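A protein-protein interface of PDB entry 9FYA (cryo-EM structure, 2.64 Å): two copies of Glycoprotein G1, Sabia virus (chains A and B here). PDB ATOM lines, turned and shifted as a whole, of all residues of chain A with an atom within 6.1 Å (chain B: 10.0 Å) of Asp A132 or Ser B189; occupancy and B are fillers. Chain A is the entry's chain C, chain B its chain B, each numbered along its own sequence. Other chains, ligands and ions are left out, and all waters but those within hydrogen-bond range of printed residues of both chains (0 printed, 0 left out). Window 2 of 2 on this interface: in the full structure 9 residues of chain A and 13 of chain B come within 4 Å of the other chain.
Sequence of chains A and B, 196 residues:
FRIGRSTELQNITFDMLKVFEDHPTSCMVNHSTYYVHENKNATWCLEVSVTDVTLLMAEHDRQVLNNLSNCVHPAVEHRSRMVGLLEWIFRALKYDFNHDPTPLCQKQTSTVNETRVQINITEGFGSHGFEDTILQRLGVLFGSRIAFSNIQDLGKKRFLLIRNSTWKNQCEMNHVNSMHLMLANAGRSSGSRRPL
OG1 of Thr A133 lies within hydrogen-bond range of OG of Ser B189, 3.2 Å away.
A ring nitrogen (NE2) of His A128 lies within hydrogen-bond range of the guanidinium group (NH2) of Arg B81, at 3.4 Å.
N of His A128 is in hydrogen-bond range of O of Ser B80, at 3.3 Å.
The side-chain hydroxyl (OG) of Ser B189 sits at hydrogen-bond distance from the backbone carbonyl oxygen (O) of Gly A129, at 2.7 Å.
The side-chain carboxylate of Glu B38 is in salt-bridge range of the guanidinium group of Arg B81 (3.3 Å).
O of Gly A129 lies within hydrogen-bond range of OG1 of Thr A133, 2.7 Å away.
His A128 touches Ser B192.
Asp A132 touches Ser B189 (CB to CB, 3.8 Å).
Thr A133 touches Gly B187.
Arg B188 touches Thr A133 (NH1 to CG2, 3.4 Å).
Of chain A, only Gly A129 (2.7 Å), Asp A132 (3.8 Å) and Thr A133 (3.2 Å) come within 4 Å of Ser B189.
No residue of chain B comes within 4 Å of Glu A131.
Of chain B, only Gly B187, Arg B188 and Ser B189 come within 4 Å of Thr A133.
No residue of chain B comes within 4 Å of Gln A136.
Printed residues of chain A within 4 Å of Ser B80: His A128.
Printed residues of chain A within 4 Å of Arg B81: His A128.
Of the printed residues of chain A, Gly B187 touches Thr A133 (3.8 Å).
Printed residues of chain A within 4 Å of Ser B192: His A128 (3.9 Å).
Printed residues of chain A within 4 Å of Arg B188: Thr A133 (3.4 Å).
Ala B186 touches none of the printed residues of chain A.
Gly B84 touches none of the printed residues of chain A.
The nearest residue of chain A that does not touch Ser B189 is Gln A136 (4.02 Å).
Of the 21 printed residues of chain B, 6 touch a printed residue of chain A.
Printed residues of chain B that touch a printed residue of chain A: Ser B80, Arg B81, Gly B187, Arg B188, Ser B189 and Ser B192.
Along chain B the printed residues that touch a printed residue of chain A span positions 80 to 192.
Of the 11 printed residues of chain A, 4 touch a printed residue of chain B.
Hydrophobic or aromatic side chains of chain A within 4 Å of the printed part of chain B: His A128.
Among the printed residues, 8 pairs touch across the chains.
Among the printed residues, no Asp or Glu carboxylate lies within 4 Å of a Lys or Arg side-chain nitrogen of the other chain.
No position is printed for both chains.
Of the 8 pairs that touch across the chains among the printed residues, none has its exchanged pair printed and touching as well.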
ATOM      1  N   HIS A 128     -14.000  -7.637  -7.425  1.00  0.00           N
ATOM      2  CA  HIS A 128     -14.766  -7.319  -8.617  1.00  0.00           C
ATOM      3  C   HIS A 128     -15.313  -5.900  -8.534  1.00  0.00           C
ATOM      4  O   HIS A 128     -15.860  -5.490  -7.508  1.00  0.00           O
ATOM      5  CB  HIS A 128     -15.909  -8.310  -8.796  1.00  0.00           C
ATOM      6  CG  HIS A 128     -16.673  -8.113 -10.065  1.00  0.00           C
ATOM      7  ND1 HIS A 128     -17.956  -7.613 -10.090  1.00  0.00           N
ATOM      8  CD2 HIS A 128     -16.333  -8.340 -11.355  1.00  0.00           C
ATOM      9  CE1 HIS A 128     -18.371  -7.537 -11.340  1.00  0.00           C
ATOM     10  NE2 HIS A 128     -17.406  -7.973 -12.127  1.00  0.00           N
ATOM     11  N   GLY A 129     -15.148  -5.145  -9.615  1.00  0.00           N
ATOM     12  CA  GLY A 129     -15.654  -3.796  -9.670  1.00  0.00           C
ATOM     13  C   GLY A 129     -14.783  -2.733  -9.043  1.00  0.00           C
ATOM     14  O   GLY A 129     -15.207  -1.576  -8.989  1.00  0.00           O
ATOM     15  N   PHE A 130     -13.597  -3.083  -8.543  1.00  0.00           N
ATOM     16  CA  PHE A 130     -12.733  -2.086  -7.920  1.00  0.00           C
ATOM     17  C   PHE A 130     -12.283  -1.031  -8.922  1.00  0.00           C
ATOM     18  O   PHE A 130     -12.279   0.167  -8.617  1.00  0.00           O
ATOM     19  CB  PHE A 130     -11.515  -2.760  -7.291  1.00  0.00           C
ATOM     20  CG  PHE A 130     -10.509  -1.788  -6.767  1.00  0.00           C
ATOM     21  CD1 PHE A 130     -10.837  -0.909  -5.752  1.00  0.00           C
ATOM     22  CD2 PHE A 130      -9.254  -1.709  -7.333  1.00  0.00           C
ATOM     23  CE1 PHE A 130      -9.917  -0.009  -5.286  1.00  0.00           C
ATOM     24  CE2 PHE A 130      -8.338  -0.803  -6.875  1.00  0.00           C
ATOM     25  CZ  PHE A 130      -8.668   0.048  -5.852  1.00  0.00           C
ATOM     26  N   GLU A 131     -11.897  -1.460 -10.123  1.00  0.00           N
ATOM     27  CA  GLU A 131     -11.534  -0.520 -11.176  1.00  0.00           C
ATOM     28  C   GLU A 131     -12.697   0.402 -11.506  1.00  0.00           C
ATOM     29  O   GLU A 131     -12.526   1.618 -11.632  1.00  0.00           O
ATOM     30  CB  GLU A 131     -11.097  -1.285 -12.423  1.00  0.00           C
ATOM     31  CG  GLU A 131     -10.659  -0.396 -13.571  1.00  0.00           C
ATOM     32  CD  GLU A 131     -10.061  -1.181 -14.720  1.00  0.00           C
ATOM     33  OE1 GLU A 131      -9.996  -2.421 -14.620  1.00  0.00           O
ATOM     34  OE2 GLU A 131      -9.660  -0.563 -15.725  1.00  0.00           O
ATOM     35  N   ASP A 132     -13.889  -0.171 -11.661  1.00  0.00           N
ATOM     36  CA  ASP A 132     -15.072   0.627 -11.947  1.00  0.00           C
ATOM     37  C   ASP A 132     -15.401   1.556 -10.789  1.00  0.00           C
ATOM     38  O   ASP A 132     -15.819   2.699 -11.002  1.00  0.00           O
ATOM     39  CB  ASP A 132     -16.242  -0.298 -12.265  1.00  0.00           C
ATOM     40  CG  ASP A 132     -15.936  -1.240 -13.411  1.00  0.00           C
ATOM     41  OD1 ASP A 132     -15.371  -0.783 -14.425  1.00  0.00           O
ATOM     42  OD2 ASP A 132     -16.249  -2.442 -13.296  1.00  0.00           O
ATOM     43  N   THR A 133     -15.210   1.087  -9.555  1.00  0.00           N
ATOM     44  CA  THR A 133     -15.448   1.933  -8.392  1.00  0.00           C
ATOM     45  C   THR A 133     -14.532   3.153  -8.415  1.00  0.00           C
ATOM     46  O   THR A 133     -14.983   4.288  -8.231  1.00  0.00           O
ATOM     47  CB  THR A 133     -15.246   1.118  -7.107  1.00  0.00           C
ATOM     48  OG1 THR A 133     -16.184   0.039  -7.073  1.00  0.00           O
ATOM     49  CG2 THR A 133     -15.466   1.970  -5.870  1.00  0.00           C
ATOM     50  N   ILE A 134     -13.244   2.936  -8.688  1.00  0.00           N
ATOM     51  CA  ILE A 134     -12.279   4.030  -8.722  1.00  0.00           C
ATOM     52  C   ILE A 134     -12.563   4.982  -9.879  1.00  0.00           C
ATOM     53  O   ILE A 134     -12.484   6.204  -9.725  1.00  0.00           O
ATOM     54  CB  ILE A 134     -10.846   3.469  -8.795  1.00  0.00           C
ATOM     55  CG1 ILE A 134     -10.480   2.763  -7.492  1.00  0.00           C
ATOM     56  CG2 ILE A 134      -9.844   4.571  -9.109  1.00  0.00           C
ATOM     57  CD1 ILE A 134     -10.404   3.668  -6.302  1.00  0.00           C
ATOM     58  N   LEU A 135     -12.882   4.444 -11.056  1.00  0.00           N
ATOM     59  CA  LEU A 135     -13.153   5.300 -12.209  1.00  0.00           C
ATOM     60  C   LEU A 135     -14.408   6.138 -12.002  1.00  0.00           C
ATOM     61  O   LEU A 135     -14.442   7.318 -12.371  1.00  0.00           O
ATOM     62  CB  LEU A 135     -13.257   4.455 -13.475  1.00  0.00           C
ATOM     63  CG  LEU A 135     -11.955   3.783 -13.925  1.00  0.00           C
ATOM     64  CD1 LEU A 135     -12.113   3.139 -15.289  1.00  0.00           C
ATOM     65  CD2 LEU A 135     -10.807   4.769 -13.929  1.00  0.00           C
ATOM     66  N   GLN A 136     -15.450   5.556 -11.408  1.00  0.00           N
ATOM     67  CA  GLN A 136     -16.634   6.346 -11.104  1.00  0.00           C
ATOM     68  C   GLN A 136     -16.361   7.371 -10.009  1.00  0.00           C
ATOM     69  O   GLN A 136     -16.947   8.459 -10.031  1.00  0.00           O
ATOM     70  CB  GLN A 136     -17.790   5.425 -10.730  1.00  0.00           C
ATOM     71  CG  GLN A 136     -18.339   4.669 -11.920  1.00  0.00           C
ATOM     72  CD  GLN A 136     -19.115   3.437 -11.531  1.00  0.00           C
ATOM     73  OE1 GLN A 136     -19.274   3.135 -10.352  1.00  0.00           O
ATOM     74  NE2 GLN A 136     -19.588   2.701 -12.524  1.00  0.00           N
ATOM     75  N   ARG A 137     -15.473   7.062  -9.055  1.00  0.00           N
ATOM     76  CA  ARG A 137     -15.063   8.087  -8.097  1.00  0.00           C
ATOM     77  C   ARG A 137     -14.338   9.229  -8.783  1.00  0.00           C
ATOM     78  O   ARG A 137     -14.485  10.385  -8.391  1.00  0.00           O
ATOM     79  CB  ARG A 137     -14.197   7.517  -6.974  1.00  0.00           C
ATOM     80  CG  ARG A 137     -14.927   6.628  -6.033  1.00  0.00           C
ATOM     81  CD  ARG A 137     -16.022   7.441  -5.355  1.00  0.00           C
ATOM     82  NE  ARG A 137     -15.514   8.623  -4.670  1.00  0.00           N
ATOM     83  CZ  ARG A 137     -16.284   9.577  -4.162  1.00  0.00           C
ATOM     84  NH1 ARG A 137     -17.602   9.518  -4.245  1.00  0.00           N
ATOM     85  NH2 ARG A 137     -15.716  10.615  -3.555  1.00  0.00           N
ATOM     86  N   ALA A 147     -14.636   6.619 -16.910  1.00  0.00           N
ATOM     87  CA  ALA A 147     -15.344   5.378 -16.614  1.00  0.00           C
ATOM     88  C   ALA A 147     -16.236   4.941 -17.769  1.00  0.00           C
ATOM     89  O   ALA A 147     -16.476   3.743 -17.946  1.00  0.00           O
ATOM     90  CB  ALA A 147     -16.181   5.533 -15.349  1.00  0.00           C
ATOM     91  N   ASP B  22     -29.827  -6.842 -11.355  1.00  0.00           N
ATOM     92  CA  ASP B  22     -28.388  -6.954 -11.522  1.00  0.00           C
ATOM     93  C   ASP B  22     -27.597  -6.459 -10.323  1.00  0.00           C
ATOM     94  O   ASP B  22     -26.375  -6.327 -10.414  1.00  0.00           O
ATOM     95  CB  ASP B  22     -27.968  -6.178 -12.770  1.00  0.00           C
ATOM     96  CG  ASP B  22     -28.536  -6.776 -14.041  1.00  0.00           C
ATOM     97  OD1 ASP B  22     -28.722  -8.007 -14.089  1.00  0.00           O
ATOM     98  OD2 ASP B  22     -28.807  -6.016 -14.989  1.00  0.00           O
ATOM     99  N   HIS B  23     -28.252  -6.180  -9.226  1.00  0.00           N
ATOM    100  CA  HIS B  23     -27.624  -5.684  -8.020  1.00  0.00           C
ATOM    101  C   HIS B  23     -27.684  -6.727  -6.913  1.00  0.00           C
ATOM    102  O   HIS B  23     -28.539  -7.617  -6.945  1.00  0.00           O
ATOM    103  CB  HIS B  23     -28.293  -4.387  -7.558  1.00  0.00           C
ATOM    104  CG  HIS B  23     -28.211  -3.292  -8.569  1.00  0.00           C
ATOM    105  ND1 HIS B  23     -27.023  -2.689  -8.912  1.00  0.00           N
ATOM    106  CD2 HIS B  23     -29.161  -2.722  -9.345  1.00  0.00           C
ATOM    107  CE1 HIS B  23     -27.247  -1.775  -9.837  1.00  0.00           C
ATOM    108  NE2 HIS B  23     -28.536  -1.777 -10.120  1.00  0.00           N
ATOM    109  N   PRO B  24     -26.762  -6.680  -5.952  1.00  0.00           N
ATOM    110  CA  PRO B  24     -26.824  -7.624  -4.835  1.00  0.00           C
ATOM    111  C   PRO B  24     -28.123  -7.473  -4.058  1.00  0.00           C
ATOM    112  O   PRO B  24     -28.639  -6.371  -3.873  1.00  0.00           O
ATOM    113  CB  PRO B  24     -25.612  -7.239  -3.984  1.00  0.00           C
ATOM    114  CG  PRO B  24     -24.673  -6.631  -4.941  1.00  0.00           C
ATOM    115  CD  PRO B  24     -25.517  -5.896  -5.930  1.00  0.00           C
ATOM    116  N   GLU B  38     -25.390 -12.161  -5.363  1.00  0.00           N
ATOM    117  CA  GLU B  38     -24.686 -11.111  -6.092  1.00  0.00           C
ATOM    118  C   GLU B  38     -25.562 -10.530  -7.195  1.00  0.00           C
ATOM    119  O   GLU B  38     -25.577  -9.315  -7.404  1.00  0.00           O
ATOM    120  CB  GLU B  38     -23.370 -11.649  -6.632  1.00  0.00           C
ATOM    121  CG  GLU B  38     -22.379 -10.583  -7.011  1.00  0.00           C
ATOM    122  CD  GLU B  38     -21.715 -10.854  -8.330  1.00  0.00           C
ATOM    123  OE1 GLU B  38     -21.941 -11.946  -8.876  1.00  0.00           O
ATOM    124  OE2 GLU B  38     -20.866 -10.036  -8.737  1.00  0.00           O
ATOM    125  N   ASN B  39     -26.267 -11.390  -7.933  1.00  0.00           N
ATOM    126  CA  ASN B  39     -27.180 -10.990  -9.002  1.00  0.00           C
ATOM    127  C   ASN B  39     -28.152 -12.144  -9.210  1.00  0.00           C
ATOM    128  O   ASN B  39     -27.897 -13.269  -8.779  1.00  0.00           O
ATOM    129  CB  ASN B  39     -26.483 -10.589 -10.320  1.00  0.00           C
ATOM    130  CG  ASN B  39     -25.574 -11.664 -10.892  1.00  0.00           C
ATOM    131  OD1 ASN B  39     -26.040 -12.611 -11.518  1.00  0.00           O
ATOM    132  ND2 ASN B  39     -24.271 -11.496 -10.717  1.00  0.00           N
ATOM    133  N   SER B  80     -13.280 -13.334  -7.577  1.00  0.00           N
ATOM    134  CA  SER B  80     -13.343 -11.884  -7.404  1.00  0.00           C
ATOM    135  C   SER B  80     -14.736 -11.421  -7.013  1.00  0.00           C
ATOM    136  O   SER B  80     -14.889 -10.562  -6.139  1.00  0.00           O
ATOM    137  CB  SER B  80     -12.898 -11.172  -8.680  1.00  0.00           C
ATOM    138  OG  SER B  80     -11.528 -11.389  -8.937  1.00  0.00           O
ATOM    139  N   ARG B  81     -15.762 -11.972  -7.656  1.00  0.00           N
ATOM    140  CA  ARG B  81     -17.129 -11.601  -7.317  1.00  0.00           C
ATOM    141  C   ARG B  81     -17.476 -12.016  -5.896  1.00  0.00           C
ATOM    142  O   ARG B  81     -18.168 -11.287  -5.182  1.00  0.00           O
ATOM    143  CB  ARG B  81     -18.102 -12.221  -8.312  1.00  0.00           C
ATOM    144  CG  ARG B  81     -17.740 -12.002  -9.759  1.00  0.00           C
ATOM    145  CD  ARG B  81     -18.991 -12.024 -10.607  1.00  0.00           C
ATOM    146  NE  ARG B  81     -18.756 -11.585 -11.976  1.00  0.00           N
ATOM    147  CZ  ARG B  81     -19.449 -10.632 -12.583  1.00  0.00           C
ATOM    148  NH1 ARG B  81     -20.426  -9.988 -11.968  1.00  0.00           N
ATOM    149  NH2 ARG B  81     -19.147 -10.312 -13.838  1.00  0.00           N
ATOM    150  N   GLY B  84     -15.860  -9.639  -3.551  1.00  0.00           N
ATOM    151  CA  GLY B  84     -16.631  -8.407  -3.596  1.00  0.00           C
ATOM    152  C   GLY B  84     -17.912  -8.476  -2.788  1.00  0.00           C
ATOM    153  O   GLY B  84     -18.270  -7.525  -2.091  1.00  0.00           O
ATOM    154  N   LEU B  85     -18.637  -9.591  -2.895  1.00  0.00           N
ATOM    155  CA  LEU B  85     -19.863  -9.753  -2.121  1.00  0.00           C
ATOM    156  C   LEU B  85     -19.566  -9.852  -0.630  1.00  0.00           C
ATOM    157  O   LEU B  85     -20.347  -9.370   0.197  1.00  0.00           O
ATOM    158  CB  LEU B  85     -20.630 -10.991  -2.585  1.00  0.00           C
ATOM    159  CG  LEU B  85     -22.144 -11.003  -2.339  1.00  0.00           C
ATOM    160  CD1 LEU B  85     -22.805  -9.737  -2.856  1.00  0.00           C
ATOM    161  CD2 LEU B  85     -22.804 -12.247  -2.891  1.00  0.00           C
ATOM    162  N   GLU B  87     -17.112  -8.270   0.868  1.00  0.00           N
ATOM    163  CA  GLU B  87     -16.898  -6.883   1.268  1.00  0.00           C
ATOM    164  C   GLU B  87     -18.213  -6.119   1.364  1.00  0.00           C
ATOM    165  O   GLU B  87     -18.380  -5.268   2.243  1.00  0.00           O
ATOM    166  CB  GLU B  87     -15.946  -6.201   0.293  1.00  0.00           C
ATOM    167  CG  GLU B  87     -14.607  -6.874   0.200  1.00  0.00           C
ATOM    168  CD  GLU B  87     -13.797  -6.391  -0.968  1.00  0.00           C
ATOM    169  OE1 GLU B  87     -14.138  -5.335  -1.528  1.00  0.00           O
ATOM    170  OE2 GLU B  87     -12.803  -7.055  -1.311  1.00  0.00           O
ATOM    171  N   TRP B  88     -19.148  -6.389   0.452  1.00  0.00           N
ATOM    172  CA  TRP B  88     -20.465  -5.765   0.540  1.00  0.00           C
ATOM    173  C   TRP B  88     -21.177  -6.145   1.832  1.00  0.00           C
ATOM    174  O   TRP B  88     -21.791  -5.296   2.482  1.00  0.00           O
ATOM    175  CB  TRP B  88     -21.305  -6.137  -0.678  1.00  0.00           C
ATOM    176  CG  TRP B  88     -21.167  -5.175  -1.811  1.00  0.00           C
ATOM    177  CD1 TRP B  88     -20.027  -4.842  -2.466  1.00  0.00           C
ATOM    178  CD2 TRP B  88     -22.220  -4.438  -2.435  1.00  0.00           C
ATOM    179  NE1 TRP B  88     -20.296  -3.930  -3.450  1.00  0.00           N
ATOM    180  CE2 TRP B  88     -21.640  -3.668  -3.456  1.00  0.00           C
ATOM    181  CE3 TRP B  88     -23.597  -4.351  -2.226  1.00  0.00           C
ATOM    182  CZ2 TRP B  88     -22.387  -2.822  -4.266  1.00  0.00           C
ATOM    183  CZ3 TRP B  88     -24.332  -3.510  -3.023  1.00  0.00           C
ATOM    184  CH2 TRP B  88     -23.729  -2.755  -4.031  1.00  0.00           C
ATOM    185  N   ARG B  91     -19.367  -4.328   4.807  1.00  0.00           N
ATOM    186  CA  ARG B  91     -19.746  -2.923   4.880  1.00  0.00           C
ATOM    187  C   ARG B  91     -21.205  -2.753   5.264  1.00  0.00           C
ATOM    188  O   ARG B  91     -21.569  -1.750   5.888  1.00  0.00           O
ATOM    189  CB  ARG B  91     -19.490  -2.243   3.538  1.00  0.00           C
ATOM    190  CG  ARG B  91     -18.041  -1.936   3.251  1.00  0.00           C
ATOM    191  CD  ARG B  91     -17.893  -1.140   1.967  1.00  0.00           C
ATOM    192  NE  ARG B  91     -16.680  -1.506   1.248  1.00  0.00           N
ATOM    193  CZ  ARG B  91     -16.635  -2.327   0.209  1.00  0.00           C
ATOM    194  NH1 ARG B  91     -17.728  -2.889  -0.276  1.00  0.00           N
ATOM    195  NH2 ARG B  91     -15.462  -2.601  -0.348  1.00  0.00           N
ATOM    196  N   MET B 182     -27.504  -1.777  -0.609  1.00  0.00           N
ATOM    197  CA  MET B 182     -26.910  -0.794  -1.508  1.00  0.00           C
ATOM    198  C   MET B 182     -26.639   0.526  -0.798  1.00  0.00           C
ATOM    199  O   MET B 182     -25.662   1.210  -1.113  1.00  0.00           O
ATOM    200  CB  MET B 182     -27.799  -0.581  -2.729  1.00  0.00           C
ATOM    201  CG  MET B 182     -27.823  -1.762  -3.676  1.00  0.00           C
ATOM    202  SD  MET B 182     -28.760  -1.431  -5.176  1.00  0.00           S
ATOM    203  CE  MET B 182     -27.707  -0.195  -5.929  1.00  0.00           C
ATOM    204  N   ASN B 185     -23.469   0.312   0.880  1.00  0.00           N
ATOM    205  CA  ASN B 185     -22.368   0.278  -0.073  1.00  0.00           C
ATOM    206  C   ASN B 185     -22.538   1.336  -1.153  1.00  0.00           C
ATOM    207  O   ASN B 185     -22.311   1.081  -2.334  1.00  0.00           O
ATOM    208  CB  ASN B 185     -22.243  -1.102  -0.712  1.00  0.00           C
ATOM    209  CG  ASN B 185     -21.944  -2.187   0.293  1.00  0.00           C
ATOM    210  OD1 ASN B 185     -20.792  -2.508   0.547  1.00  0.00           O
ATOM    211  ND2 ASN B 185     -22.990  -2.775   0.853  1.00  0.00           N
ATOM    212  N   ALA B 186     -22.952   2.536  -0.766  1.00  0.00           N
ATOM    213  CA  ALA B 186     -23.132   3.596  -1.745  1.00  0.00           C
ATOM    214  C   ALA B 186     -21.786   3.993  -2.334  1.00  0.00           C
ATOM    215  O   ALA B 186     -20.791   4.135  -1.619  1.00  0.00           O
ATOM    216  CB  ALA B 186     -23.816   4.800  -1.106  1.00  0.00           C
ATOM    217  N   GLY B 187     -21.767   4.201  -3.643  1.00  0.00           N
ATOM    218  CA  GLY B 187     -20.566   4.572  -4.349  1.00  0.00           C
ATOM    219  C   GLY B 187     -19.774   3.419  -4.917  1.00  0.00           C
ATOM    220  O   GLY B 187     -18.860   3.655  -5.711  1.00  0.00           O
ATOM    221  N   ARG B 188     -20.099   2.180  -4.555  1.00  0.00           N
ATOM    222  CA  ARG B 188     -19.426   1.027  -5.130  1.00  0.00           C
ATOM    223  C   ARG B 188     -20.015   0.741  -6.504  1.00  0.00           C
ATOM    224  O   ARG B 188     -20.932   1.420  -6.966  1.00  0.00           O
ATOM    225  CB  ARG B 188     -19.526  -0.161  -4.179  1.00  0.00           C
ATOM    226  CG  ARG B 188     -18.742   0.042  -2.907  1.00  0.00           C
ATOM    227  CD  ARG B 188     -17.296  -0.319  -3.205  1.00  0.00           C
ATOM    228  NE  ARG B 188     -16.371  -0.045  -2.118  1.00  0.00           N
ATOM    229  CZ  ARG B 188     -15.057   0.043  -2.266  1.00  0.00           C
ATOM    230  NH1 ARG B 188     -14.479  -0.150  -3.436  1.00  0.00           N
ATOM    231  NH2 ARG B 188     -14.306   0.358  -1.218  1.00  0.00           N
ATOM    232  N   SER B 189     -19.514  -0.288  -7.165  1.00  0.00           N
ATOM    233  CA  SER B 189     -19.948  -0.603  -8.515  1.00  0.00           C
ATOM    234  C   SER B 189     -20.780  -1.871  -8.492  1.00  0.00           C
ATOM    235  O   SER B 189     -20.370  -2.879  -7.911  1.00  0.00           O
ATOM    236  CB  SER B 189     -18.754  -0.750  -9.459  1.00  0.00           C
ATOM    237  OG  SER B 189     -17.918  -1.816  -9.060  1.00  0.00           O
ATOM    238  N   SER B 190     -21.957  -1.804  -9.100  1.00  0.00           N
ATOM    239  CA  SER B 190     -22.848  -2.946  -9.189  1.00  0.00           C
ATOM    240  C   SER B 190     -23.670  -2.817 -10.459  1.00  0.00           C
ATOM    241  O   SER B 190     -24.068  -1.715 -10.840  1.00  0.00           O
ATOM    242  CB  SER B 190     -23.754  -3.045  -7.956  1.00  0.00           C
ATOM    243  OG  SER B 190     -24.613  -1.927  -7.849  1.00  0.00           O
ATOM    244  N   GLY B 191     -23.879  -3.939 -11.131  1.00  0.00           N
ATOM    245  CA  GLY B 191     -24.617  -3.958 -12.374  1.00  0.00           C
ATOM    246  C   GLY B 191     -23.724  -4.219 -13.567  1.00  0.00           C
ATOM    247  O   GLY B 191     -22.985  -3.334 -14.005  1.00  0.00           O
ATOM    248  N   SER B 192     -23.775  -5.435 -14.094  1.00  0.00           N
ATOM    249  CA  SER B 192     -22.963  -5.804 -15.245  1.00  0.00           C
ATOM    250  C   SER B 192     -23.848  -6.126 -16.444  1.00  0.00           C
ATOM    251  O   SER B 192     -24.723  -6.991 -16.365  1.00  0.00           O
ATOM    252  CB  SER B 192     -22.056  -6.986 -14.909  1.00  0.00           C
ATOM    253  OG  SER B 192     -21.115  -6.629 -13.908  1.00  0.00           O
